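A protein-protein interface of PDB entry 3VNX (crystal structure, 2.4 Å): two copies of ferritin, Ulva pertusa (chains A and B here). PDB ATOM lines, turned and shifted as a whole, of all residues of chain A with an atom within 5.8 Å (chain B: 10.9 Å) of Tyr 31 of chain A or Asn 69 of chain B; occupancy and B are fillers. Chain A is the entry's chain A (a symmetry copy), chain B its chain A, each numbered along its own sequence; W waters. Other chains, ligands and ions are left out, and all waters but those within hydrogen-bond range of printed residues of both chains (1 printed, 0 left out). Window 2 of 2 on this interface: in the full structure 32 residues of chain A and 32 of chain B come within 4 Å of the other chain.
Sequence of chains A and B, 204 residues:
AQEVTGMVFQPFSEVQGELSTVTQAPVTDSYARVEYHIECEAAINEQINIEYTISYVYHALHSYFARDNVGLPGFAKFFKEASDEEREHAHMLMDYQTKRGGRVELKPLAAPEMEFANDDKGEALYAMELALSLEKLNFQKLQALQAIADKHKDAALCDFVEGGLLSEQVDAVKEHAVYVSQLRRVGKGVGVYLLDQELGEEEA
ND2 of Asn 69 of chain B touches C of Thr 28 of chain A (3.9 Å).
Ser 30 of chain A touches Asn 69 of chain B (CA to OD1, 3.5 Å).
CE2 of Tyr 31 of chain A touches CB of Asn 69 of chain B, at 3.9 Å.
Arg 103 of chain A touches Arg 67 of chain B.
The side-chain carboxylate (OE1) of Glu 115 of chain B is in salt-bridge range of the guanidinium group (NH2) of Arg 67 of chain B.
The guanidinium group of Arg 103 of chain A sits at hydrogen-bond distance from the backbone carbonyl oxygen of Thr 28 of chain A.
N of Ala 32 of chain A is in hydrogen-bond range of OG of Ser 30 of chain A (3.1 Å).
The side-chain hydroxyl (OG) of Ser 30 of chain A sits at hydrogen-bond distance from the backbone NH (N) of Arg 33 of chain A, at 3.1 Å.
Of the 21 printed residues of chain B, 3 touch a printed residue of chain A.
Printed residues of chain A that touch a printed residue of chain B: Val 27, Thr 28, Asp 29, Ser 30, Tyr 31, Ala 32 and Arg 103.
Hydrophobic or aromatic side chains of chain A that line the printed part of chain B: Tyr 31 and Ala 32.
Along chain A the printed residues that touch a printed residue of chain B span positions 27 to 103.
The side-chain carboxylate (OD2) of Asp 68 of chain B lies within hydrogen-bond range of the side-chain hydroxyl (OG) of Ser 30 of chain A (2.9 Å).
The side-chain carboxylate (OD1) of Asp 68 of chain B is in hydrogen-bond range of the backbone NH (N) of Tyr 31 of chain A (2.6 Å).
The side-chain carboxylate of Asp 68 of chain B sits at hydrogen-bond distance from the backbone NH of Ala 32 of chain A (3.2 Å).
O of Val 27 of chain A is in hydrogen-bond range of ND2 of Asn 69 of chain B, at 3.0 Å.
ND2 of Asn 69 of chain B lies close to O of Asp 29 of chain A (3.4 Å).
Water W1 bridges the guanidinium group of Arg 103 of chain A (2.7 Å) and the side-chain amide oxygen of Asn 69 of chain B (2.7 Å).
No position is printed for both chains.
No residue of chain B comes within 4 Å of Ala 25 of chain A.
No residue of chain B comes within 4 Å of Pro 26 of chain A.
Thr 28 of chain A touches just one residue of chain B: Asn 69.
Printed residues of chain B within 4 Å of Asp 29 of chain A: Asn 69.
Ser 30 of chain A touches two residues of chain B.
Tyr 31 of chain A touches just these residues of chain B: Asp 68 (2.6 Å) and Asn 69 (3.9 Å).
Ala 32 of chain A touches one residue of chain B.
Printed residues of chain B within 4 Å of Arg 103 of chain A: Arg 67 (3.3 Å).
Tyr 64 of chain B touches none of the printed residues of chain A.
Of the printed residues of chain A, Arg 67 of chain B touches Arg 103.
Printed residues of chain A within 4 Å of Asp 68 of chain B: Ser 30 (2.9 Å), Tyr 31 (2.6 Å) and Ala 32 (3.2 Å).
Asn 69 of chain B touches five residues of chain A.
The nearest printed residue of chain A that does not touch Asp 68 of chain B is Arg 33 of chain A (4.9 Å).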
ATOM      1  N   VAL A  22      -6.223   0.392   5.491  1.00  0.00           N
ATOM      2  CA  VAL A  22      -5.805   1.782   5.480  1.00  0.00           C
ATOM      3  C   VAL A  22      -6.344   2.566   6.678  1.00  0.00           C
ATOM      4  O   VAL A  22      -5.587   3.298   7.337  1.00  0.00           O
ATOM      5  CB  VAL A  22      -6.216   2.486   4.157  1.00  0.00           C
ATOM      6  CG1 VAL A  22      -6.189   4.009   4.321  1.00  0.00           C
ATOM      7  CG2 VAL A  22      -5.315   2.028   3.000  1.00  0.00           C
ATOM      8  N   ALA A  25      -4.587   1.439  10.022  1.00  0.00           N
ATOM      9  CA  ALA A  25      -3.131   1.545  10.138  1.00  0.00           C
ATOM     10  C   ALA A  25      -2.676   2.635  11.108  1.00  0.00           C
ATOM     11  O   ALA A  25      -3.238   3.737  11.135  1.00  0.00           O
ATOM     12  CB  ALA A  25      -2.480   1.737   8.760  1.00  0.00           C
ATOM     13  N   PRO A  26      -1.672   2.310  11.937  1.00  0.00           N
ATOM     14  CA  PRO A  26      -1.017   3.296  12.805  1.00  0.00           C
ATOM     15  C   PRO A  26      -0.017   4.141  12.001  1.00  0.00           C
ATOM     16  O   PRO A  26       0.433   3.748  10.911  1.00  0.00           O
ATOM     17  CB  PRO A  26      -0.280   2.422  13.828  1.00  0.00           C
ATOM     18  CG  PRO A  26       0.002   1.139  13.094  1.00  0.00           C
ATOM     19  CD  PRO A  26      -1.152   0.944  12.147  1.00  0.00           C
ATOM     20  N   VAL A  27       0.340   5.301  12.532  1.00  0.00           N
ATOM     21  CA  VAL A  27       1.208   6.190  11.778  1.00  0.00           C
ATOM     22  C   VAL A  27       2.621   5.634  11.701  1.00  0.00           C
ATOM     23  O   VAL A  27       3.518   6.280  11.165  1.00  0.00           O
ATOM     24  CB  VAL A  27       1.209   7.596  12.383  1.00  0.00           C
ATOM     25  CG1 VAL A  27      -0.223   8.119  12.435  1.00  0.00           C
ATOM     26  CG2 VAL A  27       1.871   7.597  13.797  1.00  0.00           C
ATOM     27  N   THR A  28       2.812   4.436  12.244  1.00  0.00           N
ATOM     28  CA  THR A  28       4.137   3.827  12.316  1.00  0.00           C
ATOM     29  C   THR A  28       4.312   2.858  11.170  1.00  0.00           C
ATOM     30  O   THR A  28       5.418   2.391  10.914  1.00  0.00           O
ATOM     31  CB  THR A  28       4.344   3.032  13.625  1.00  0.00           C
ATOM     32  OG1 THR A  28       3.229   2.151  13.843  1.00  0.00           O
ATOM     33  CG2 THR A  28       4.476   3.965  14.792  1.00  0.00           C
ATOM     34  N   ASP A  29       3.200   2.544  10.510  1.00  0.00           N
ATOM     35  CA  ASP A  29       3.202   1.671   9.345  1.00  0.00           C
ATOM     36  C   ASP A  29       3.240   2.485   8.056  1.00  0.00           C
ATOM     37  O   ASP A  29       2.634   3.556   7.973  1.00  0.00           O
ATOM     38  CB  ASP A  29       1.942   0.799   9.331  1.00  0.00           C
ATOM     39  CG  ASP A  29       2.008  -0.355  10.319  1.00  0.00           C
ATOM     40  OD1 ASP A  29       1.021  -1.123  10.387  1.00  0.00           O
ATOM     41  OD2 ASP A  29       3.033  -0.491  11.024  1.00  0.00           O
ATOM     42  N   SER A  30       3.961   1.978   7.059  1.00  0.00           N
ATOM     43  CA  SER A  30       3.854   2.504   5.709  1.00  0.00           C
ATOM     44  C   SER A  30       2.416   2.288   5.264  1.00  0.00           C
ATOM     45  O   SER A  30       1.833   1.229   5.517  1.00  0.00           O
ATOM     46  CB  SER A  30       4.791   1.742   4.772  1.00  0.00           C
ATOM     47  OG  SER A  30       4.278   1.726   3.450  1.00  0.00           O
ATOM     48  N   TYR A  31       1.830   3.279   4.607  1.00  0.00           N
ATOM     49  CA  TYR A  31       0.484   3.103   4.083  1.00  0.00           C
ATOM     50  C   TYR A  31       0.522   2.567   2.663  1.00  0.00           C
ATOM     51  O   TYR A  31      -0.498   2.138   2.127  1.00  0.00           O
ATOM     52  CB  TYR A  31      -0.276   4.424   4.074  1.00  0.00           C
ATOM     53  CG  TYR A  31      -0.293   5.158   5.386  1.00  0.00           C
ATOM     54  CD1 TYR A  31      -0.390   4.471   6.597  1.00  0.00           C
ATOM     55  CD2 TYR A  31      -0.235   6.550   5.417  1.00  0.00           C
ATOM     56  CE1 TYR A  31      -0.419   5.159   7.801  1.00  0.00           C
ATOM     57  CE2 TYR A  31      -0.255   7.244   6.616  1.00  0.00           C
ATOM     58  CZ  TYR A  31      -0.349   6.550   7.803  1.00  0.00           C
ATOM     59  OH  TYR A  31      -0.372   7.257   8.987  1.00  0.00           O
ATOM     60  N   ALA A  32       1.699   2.620   2.047  1.00  0.00           N
ATOM     61  CA  ALA A  32       1.813   2.376   0.611  1.00  0.00           C
ATOM     62  C   ALA A  32       2.122   0.914   0.281  1.00  0.00           C
ATOM     63  O   ALA A  32       1.686   0.393  -0.751  1.00  0.00           O
ATOM     64  CB  ALA A  32       2.883   3.300  -0.004  1.00  0.00           C
ATOM     65  N   ARG A  33       2.869   0.260   1.165  1.00  0.00           N
ATOM     66  CA  ARG A  33       3.410  -1.069   0.888  1.00  0.00           C
ATOM     67  C   ARG A  33       2.371  -2.079   0.393  1.00  0.00           C
ATOM     68  O   ARG A  33       1.365  -2.318   1.053  1.00  0.00           O
ATOM     69  CB  ARG A  33       4.117  -1.604   2.124  1.00  0.00           C
ATOM     70  CG  ARG A  33       5.012  -2.787   1.845  1.00  0.00           C
ATOM     71  CD  ARG A  33       5.778  -3.173   3.098  1.00  0.00           C
ATOM     72  NE  ARG A  33       6.736  -4.226   2.806  1.00  0.00           N
ATOM     73  CZ  ARG A  33       7.969  -4.275   3.292  1.00  0.00           C
ATOM     74  NH1 ARG A  33       8.407  -3.322   4.105  1.00  0.00           N
ATOM     75  NH2 ARG A  33       8.769  -5.277   2.952  1.00  0.00           N
ATOM     76  N   ARG A 103      11.692   0.218   3.897  1.00  0.00           N
ATOM     77  CA  ARG A 103      12.494   1.171   4.663  1.00  0.00           C
ATOM     78  C   ARG A 103      13.991   1.054   4.380  1.00  0.00           C
ATOM     79  O   ARG A 103      14.552  -0.041   4.341  1.00  0.00           O
ATOM     80  CB  ARG A 103      12.181   1.086   6.160  1.00  0.00           C
ATOM     81  CG  ARG A 103      10.689   1.151   6.400  1.00  0.00           C
ATOM     82  CD  ARG A 103      10.285   1.718   7.756  1.00  0.00           C
ATOM     83  NE  ARG A 103       8.829   1.894   7.798  1.00  0.00           N
ATOM     84  CZ  ARG A 103       8.044   1.504   8.803  1.00  0.00           C
ATOM     85  NH1 ARG A 103       8.578   0.927   9.871  1.00  0.00           N
ATOM     86  NH2 ARG A 103       6.723   1.698   8.743  1.00  0.00           N
ATOM     87  N   HIS B  62      17.038  12.014   5.463  1.00  0.00           N
ATOM     88  CA  HIS B  62      16.273  12.201   4.250  1.00  0.00           C
ATOM     89  C   HIS B  62      15.340  11.015   4.006  1.00  0.00           C
ATOM     90  O   HIS B  62      14.141  11.188   3.715  1.00  0.00           O
ATOM     91  CB  HIS B  62      17.200  12.386   3.053  1.00  0.00           C
ATOM     92  CG  HIS B  62      16.538  12.085   1.750  1.00  0.00           C
ATOM     93  ND1 HIS B  62      15.671  12.964   1.136  1.00  0.00           N
ATOM     94  CD2 HIS B  62      16.586  10.985   0.958  1.00  0.00           C
ATOM     95  CE1 HIS B  62      15.228  12.426   0.012  1.00  0.00           C
ATOM     96  NE2 HIS B  62      15.768  11.226  -0.118  1.00  0.00           N
ATOM     97  N   SER B  63      15.889   9.807   4.107  1.00  0.00           N
ATOM     98  CA  SER B  63      15.085   8.621   3.834  1.00  0.00           C
ATOM     99  C   SER B  63      13.960   8.486   4.841  1.00  0.00           C
ATOM    100  O   SER B  63      12.881   7.984   4.522  1.00  0.00           O
ATOM    101  CB  SER B  63      15.945   7.359   3.805  1.00  0.00           C
ATOM    102  OG  SER B  63      16.602   7.254   2.554  1.00  0.00           O
ATOM    103  N   TYR B  64      14.206   8.945   6.059  1.00  0.00           N
ATOM    104  CA  TYR B  64      13.159   8.882   7.063  1.00  0.00           C
ATOM    105  C   TYR B  64      11.957   9.755   6.641  1.00  0.00           C
ATOM    106  O   TYR B  64      10.816   9.281   6.604  1.00  0.00           O
ATOM    107  CB  TYR B  64      13.683   9.230   8.472  1.00  0.00           C
ATOM    108  CG  TYR B  64      12.567   9.243   9.485  1.00  0.00           C
ATOM    109  CD1 TYR B  64      12.121   8.056  10.076  1.00  0.00           C
ATOM    110  CD2 TYR B  64      11.914  10.434   9.816  1.00  0.00           C
ATOM    111  CE1 TYR B  64      11.079   8.056  10.983  1.00  0.00           C
ATOM    112  CE2 TYR B  64      10.863  10.442  10.726  1.00  0.00           C
ATOM    113  CZ  TYR B  64      10.450   9.252  11.306  1.00  0.00           C
ATOM    114  OH  TYR B  64       9.404   9.256  12.207  1.00  0.00           O
ATOM    115  N   PHE B  65      12.217  11.011   6.284  1.00  0.00           N
ATOM    116  CA  PHE B  65      11.135  11.919   5.907  1.00  0.00           C
ATOM    117  C   PHE B  65      10.515  11.608   4.542  1.00  0.00           C
ATOM    118  O   PHE B  65       9.378  12.008   4.261  1.00  0.00           O
ATOM    119  CB  PHE B  65      11.581  13.379   6.014  1.00  0.00           C
ATOM    120  CG  PHE B  65      11.858  13.801   7.418  1.00  0.00           C
ATOM    121  CD1 PHE B  65      10.813  14.146   8.270  1.00  0.00           C
ATOM    122  CD2 PHE B  65      13.155  13.800   7.915  1.00  0.00           C
ATOM    123  CE1 PHE B  65      11.056  14.519   9.594  1.00  0.00           C
ATOM    124  CE2 PHE B  65      13.410  14.167   9.223  1.00  0.00           C
ATOM    125  CZ  PHE B  65      12.352  14.527  10.073  1.00  0.00           C
ATOM    126  N   ALA B  66      11.246  10.859   3.719  1.00  0.00           N
ATOM    127  CA  ALA B  66      10.699  10.344   2.462  1.00  0.00           C
ATOM    128  C   ALA B  66       9.645   9.245   2.654  1.00  0.00           C
ATOM    129  O   ALA B  66       8.878   8.969   1.733  1.00  0.00           O
ATOM    130  CB  ALA B  66      11.819   9.835   1.552  1.00  0.00           C
ATOM    131  N   ARG B  67       9.599   8.610   3.826  1.00  0.00           N
ATOM    132  CA  ARG B  67       8.628   7.521   4.019  1.00  0.00           C
ATOM    133  C   ARG B  67       7.193   8.001   3.862  1.00  0.00           C
ATOM    134  O   ARG B  67       6.794   8.992   4.458  1.00  0.00           O
ATOM    135  CB  ARG B  67       8.775   6.875   5.386  1.00  0.00           C
ATOM    136  CG  ARG B  67      10.149   6.357   5.654  1.00  0.00           C
ATOM    137  CD  ARG B  67      10.218   5.855   7.058  1.00  0.00           C
ATOM    138  NE  ARG B  67      11.481   5.186   7.328  1.00  0.00           N
ATOM    139  CZ  ARG B  67      11.780   4.618   8.488  1.00  0.00           C
ATOM    140  NH1 ARG B  67      10.903   4.633   9.485  1.00  0.00           N
ATOM    141  NH2 ARG B  67      12.956   4.035   8.646  1.00  0.00           N
ATOM    142  N   ASP B  68       6.419   7.278   3.067  1.00  0.00           N
ATOM    143  CA  ASP B  68       5.062   7.697   2.746  1.00  0.00           C
ATOM    144  C   ASP B  68       4.217   8.064   3.966  1.00  0.00           C
ATOM    145  O   ASP B  68       3.362   8.940   3.892  1.00  0.00           O
ATOM    146  CB  ASP B  68       4.359   6.622   1.911  1.00  0.00           C
ATOM    147  CG  ASP B  68       4.098   5.349   2.695  1.00  0.00           C
ATOM    148  OD1 ASP B  68       3.019   5.240   3.322  1.00  0.00           O
ATOM    149  OD2 ASP B  68       4.965   4.455   2.669  1.00  0.00           O
ATOM    150  N   ASN B  69       4.440   7.396   5.091  1.00  0.00           N
ATOM    151  CA  ASN B  69       3.597   7.638   6.263  1.00  0.00           C
ATOM    152  C   ASN B  69       4.100   8.804   7.112  1.00  0.00           C
ATOM    153  O   ASN B  69       3.382   9.316   7.989  1.00  0.00           O
ATOM    154  CB  ASN B  69       3.481   6.377   7.108  1.00  0.00           C
ATOM    155  CG  ASN B  69       4.828   5.783   7.416  1.00  0.00           C
ATOM    156  OD1 ASN B  69       5.572   5.409   6.507  1.00  0.00           O
ATOM    157  ND2 ASN B  69       5.165   5.712   8.691  1.00  0.00           N
ATOM    158  N   VAL B  70       5.340   9.213   6.848  1.00  0.00           N
ATOM    159  CA  VAL B  70       5.894  10.423   7.443  1.00  0.00           C
ATOM    160  C   VAL B  70       5.428  11.654   6.644  1.00  0.00           C
ATOM    161  O   VAL B  70       5.012  12.664   7.229  1.00  0.00           O
ATOM    162  CB  VAL B  70       7.425  10.340   7.559  1.00  0.00           C
ATOM    163  CG1 VAL B  70       8.005  11.629   8.153  1.00  0.00           C
ATOM    164  CG2 VAL B  70       7.814   9.137   8.409  1.00  0.00           C
ATOM    165  N   GLY B  71       5.448  11.547   5.316  1.00  0.00           N
ATOM    166  CA  GLY B  71       4.849  12.558   4.456  1.00  0.00           C
ATOM    167  C   GLY B  71       5.369  13.964   4.723  1.00  0.00           C
ATOM    168  O   GLY B  71       4.588  14.882   4.922  1.00  0.00           O
ATOM    169  N   LEU B  72       6.692  14.127   4.739  1.00  0.00           N
ATOM    170  CA  LEU B  72       7.320  15.432   4.942  1.00  0.00           C
ATOM    171  C   LEU B  72       8.440  15.631   3.915  1.00  0.00           C
ATOM    172  O   LEU B  72       9.620  15.716   4.272  1.00  0.00           O
ATOM    173  CB  LEU B  72       7.868  15.555   6.369  1.00  0.00           C
ATOM    174  CG  LEU B  72       6.837  15.804   7.474  1.00  0.00           C
ATOM    175  CD1 LEU B  72       7.514  15.814   8.859  1.00  0.00           C
ATOM    176  CD2 LEU B  72       6.068  17.099   7.212  1.00  0.00           C
ATOM    177  N   PRO B  73       8.059  15.701   2.630  1.00  0.00           N
ATOM    178  CA  PRO B  73       8.998  15.710   1.498  1.00  0.00           C
ATOM    179  C   PRO B  73       9.863  16.977   1.445  1.00  0.00           C
ATOM    180  O   PRO B  73      10.960  16.923   0.882  1.00  0.00           O
ATOM    181  CB  PRO B  73       8.083  15.582   0.261  1.00  0.00           C
ATOM    182  CG  PRO B  73       6.719  16.059   0.725  1.00  0.00           C
ATOM    183  CD  PRO B  73       6.645  15.783   2.205  1.00  0.00           C
ATOM    184  N   ALA B  76      12.537  16.105   3.699  1.00  0.00           N
ATOM    185  CA  ALA B  76      13.329  15.138   2.955  1.00  0.00           C
ATOM    186  C   ALA B  76      14.284  15.843   1.983  1.00  0.00           C
ATOM    187  O   ALA B  76      15.462  15.490   1.880  1.00  0.00           O
ATOM    188  CB  ALA B  76      12.439  14.134   2.226  1.00  0.00           C
ATOM    189  N   MET B 114      18.399   5.215  11.652  1.00  0.00           N
ATOM    190  CA  MET B 114      17.410   5.360  10.586  1.00  0.00           C
ATOM    191  C   MET B 114      16.047   5.822  11.102  1.00  0.00           C
ATOM    192  O   MET B 114      15.178   6.232  10.322  1.00  0.00           O
ATOM    193  CB  MET B 114      17.235   4.039   9.823  1.00  0.00           C
ATOM    194  CG  MET B 114      18.552   3.364   9.414  1.00  0.00           C
ATOM    195  SD  MET B 114      19.657   4.357   8.372  1.00  0.00           S
ATOM    196  CE  MET B 114      18.538   4.869   7.085  1.00  0.00           C
ATOM    197  N   GLU B 115      15.864   5.753  12.413  1.00  0.00           N
ATOM    198  CA  GLU B 115      14.549   5.966  13.009  1.00  0.00           C
ATOM    199  C   GLU B 115      14.519   7.261  13.777  1.00  0.00           C
ATOM    200  O   GLU B 115      15.416   7.536  14.578  1.00  0.00           O
ATOM    201  CB  GLU B 115      14.210   4.805  13.942  1.00  0.00           C
ATOM    202  CG  GLU B 115      14.228   3.477  13.232  1.00  0.00           C
ATOM    203  CD  GLU B 115      13.219   3.434  12.111  1.00  0.00           C
ATOM    204  OE1 GLU B 115      13.429   2.658  11.147  1.00  0.00           O
ATOM    205  OE2 GLU B 115      12.214   4.183  12.198  1.00  0.00           O
ATOM    206  N   PHE B 116      13.493   8.070  13.547  1.00  0.00           N
ATOM    207  CA  PHE B 116      13.503   9.405  14.152  1.00  0.00           C
ATOM    208  C   PHE B 116      12.165   9.833  14.727  1.00  0.00           C
ATOM    209  O   PHE B 116      11.967  11.009  15.049  1.00  0.00           O
ATOM    210  CB  PHE B 116      14.079  10.450  13.181  1.00  0.00           C
ATOM    211  CG  PHE B 116      15.468  10.127  12.721  1.00  0.00           C
ATOM    212  CD1 PHE B 116      15.678   9.468  11.521  1.00  0.00           C
ATOM    213  CD2 PHE B 116      16.565  10.443  13.514  1.00  0.00           C
ATOM    214  CE1 PHE B 116      16.969   9.146  11.100  1.00  0.00           C
ATOM    215  CE2 PHE B 116      17.853  10.127  13.109  1.00  0.00           C
ATOM    216  CZ  PHE B 116      18.059   9.470  11.902  1.00  0.00           C
ATOM    217  N   ALA B 117      11.259   8.870  14.864  1.00  0.00           N
ATOM    218  CA  ALA B 117      10.013   9.101  15.572  1.00  0.00           C
ATOM    219  C   ALA B 117      10.333   9.554  16.997  1.00  0.00           C
ATOM    220  O   ALA B 117      11.309   9.113  17.607  1.00  0.00           O
ATOM    221  CB  ALA B 117       9.148   7.838  15.579  1.00  0.00           C
ATOM    222  N   GLU B 123       8.752  14.172  15.336  1.00  0.00           N
ATOM    223  CA  GLU B 123       9.962  13.876  14.554  1.00  0.00           C
ATOM    224  C   GLU B 123      10.568  15.121  13.883  1.00  0.00           C
ATOM    225  O   GLU B 123      11.794  15.242  13.769  1.00  0.00           O
ATOM    226  CB  GLU B 123       9.739  12.774  13.509  1.00  0.00           C
ATOM    227  CG  GLU B 123       8.338  12.176  13.466  1.00  0.00           C
ATOM    228  CD  GLU B 123       7.327  13.088  12.798  1.00  0.00           C
ATOM    229  OE1 GLU B 123       7.641  14.286  12.609  1.00  0.00           O
ATOM    230  OE2 GLU B 123       6.219  12.610  12.469  1.00  0.00           O
ATOM    231  N   ALA B 124       9.720  16.037  13.431  1.00  0.00           N
ATOM    232  CA  ALA B 124      10.233  17.238  12.791  1.00  0.00           C
ATOM    233  C   ALA B 124      11.182  17.921  13.757  1.00  0.00           C
ATOM    234  O   ALA B 124      12.402  17.990  13.522  1.00  0.00           O
ATOM    235  CB  ALA B 124       9.094  18.176  12.397  1.00  0.00           C
ATOM    236  N   VAL B 192       4.135  22.062  11.536  1.00  0.00           N
ATOM    237  CA  VAL B 192       5.096  21.200  10.854  1.00  0.00           C
ATOM    238  C   VAL B 192       4.818  21.157   9.347  1.00  0.00           C
ATOM    239  O   VAL B 192       5.736  21.208   8.522  1.00  0.00           O
ATOM    240  CB  VAL B 192       5.098  19.764  11.457  1.00  0.00           C
ATOM    241  CG1 VAL B 192       5.994  18.834  10.643  1.00  0.00           C
ATOM    242  CG2 VAL B 192       5.521  19.788  12.965  1.00  0.00           C
ATOM    243  N   ASP B 196       7.456  22.370   6.693  1.00  0.00           N
ATOM    244  CA  ASP B 196       7.836  21.431   5.651  1.00  0.00           C
ATOM    245  C   ASP B 196       7.682  22.089   4.275  1.00  0.00           C
ATOM    246  O   ASP B 196       8.493  21.870   3.380  1.00  0.00           O
ATOM    247  CB  ASP B 196       7.007  20.152   5.709  1.00  0.00           C
ATOM    248  CG  ASP B 196       7.331  19.204   4.554  1.00  0.00           C
ATOM    249  OD1 ASP B 196       8.346  18.482   4.649  1.00  0.00           O
ATOM    250  OD2 ASP B 196       6.593  19.188   3.543  1.00  0.00           O
HETATM  251  O   HOH W   1       7.404   3.481   6.195  1.00  0.00           O
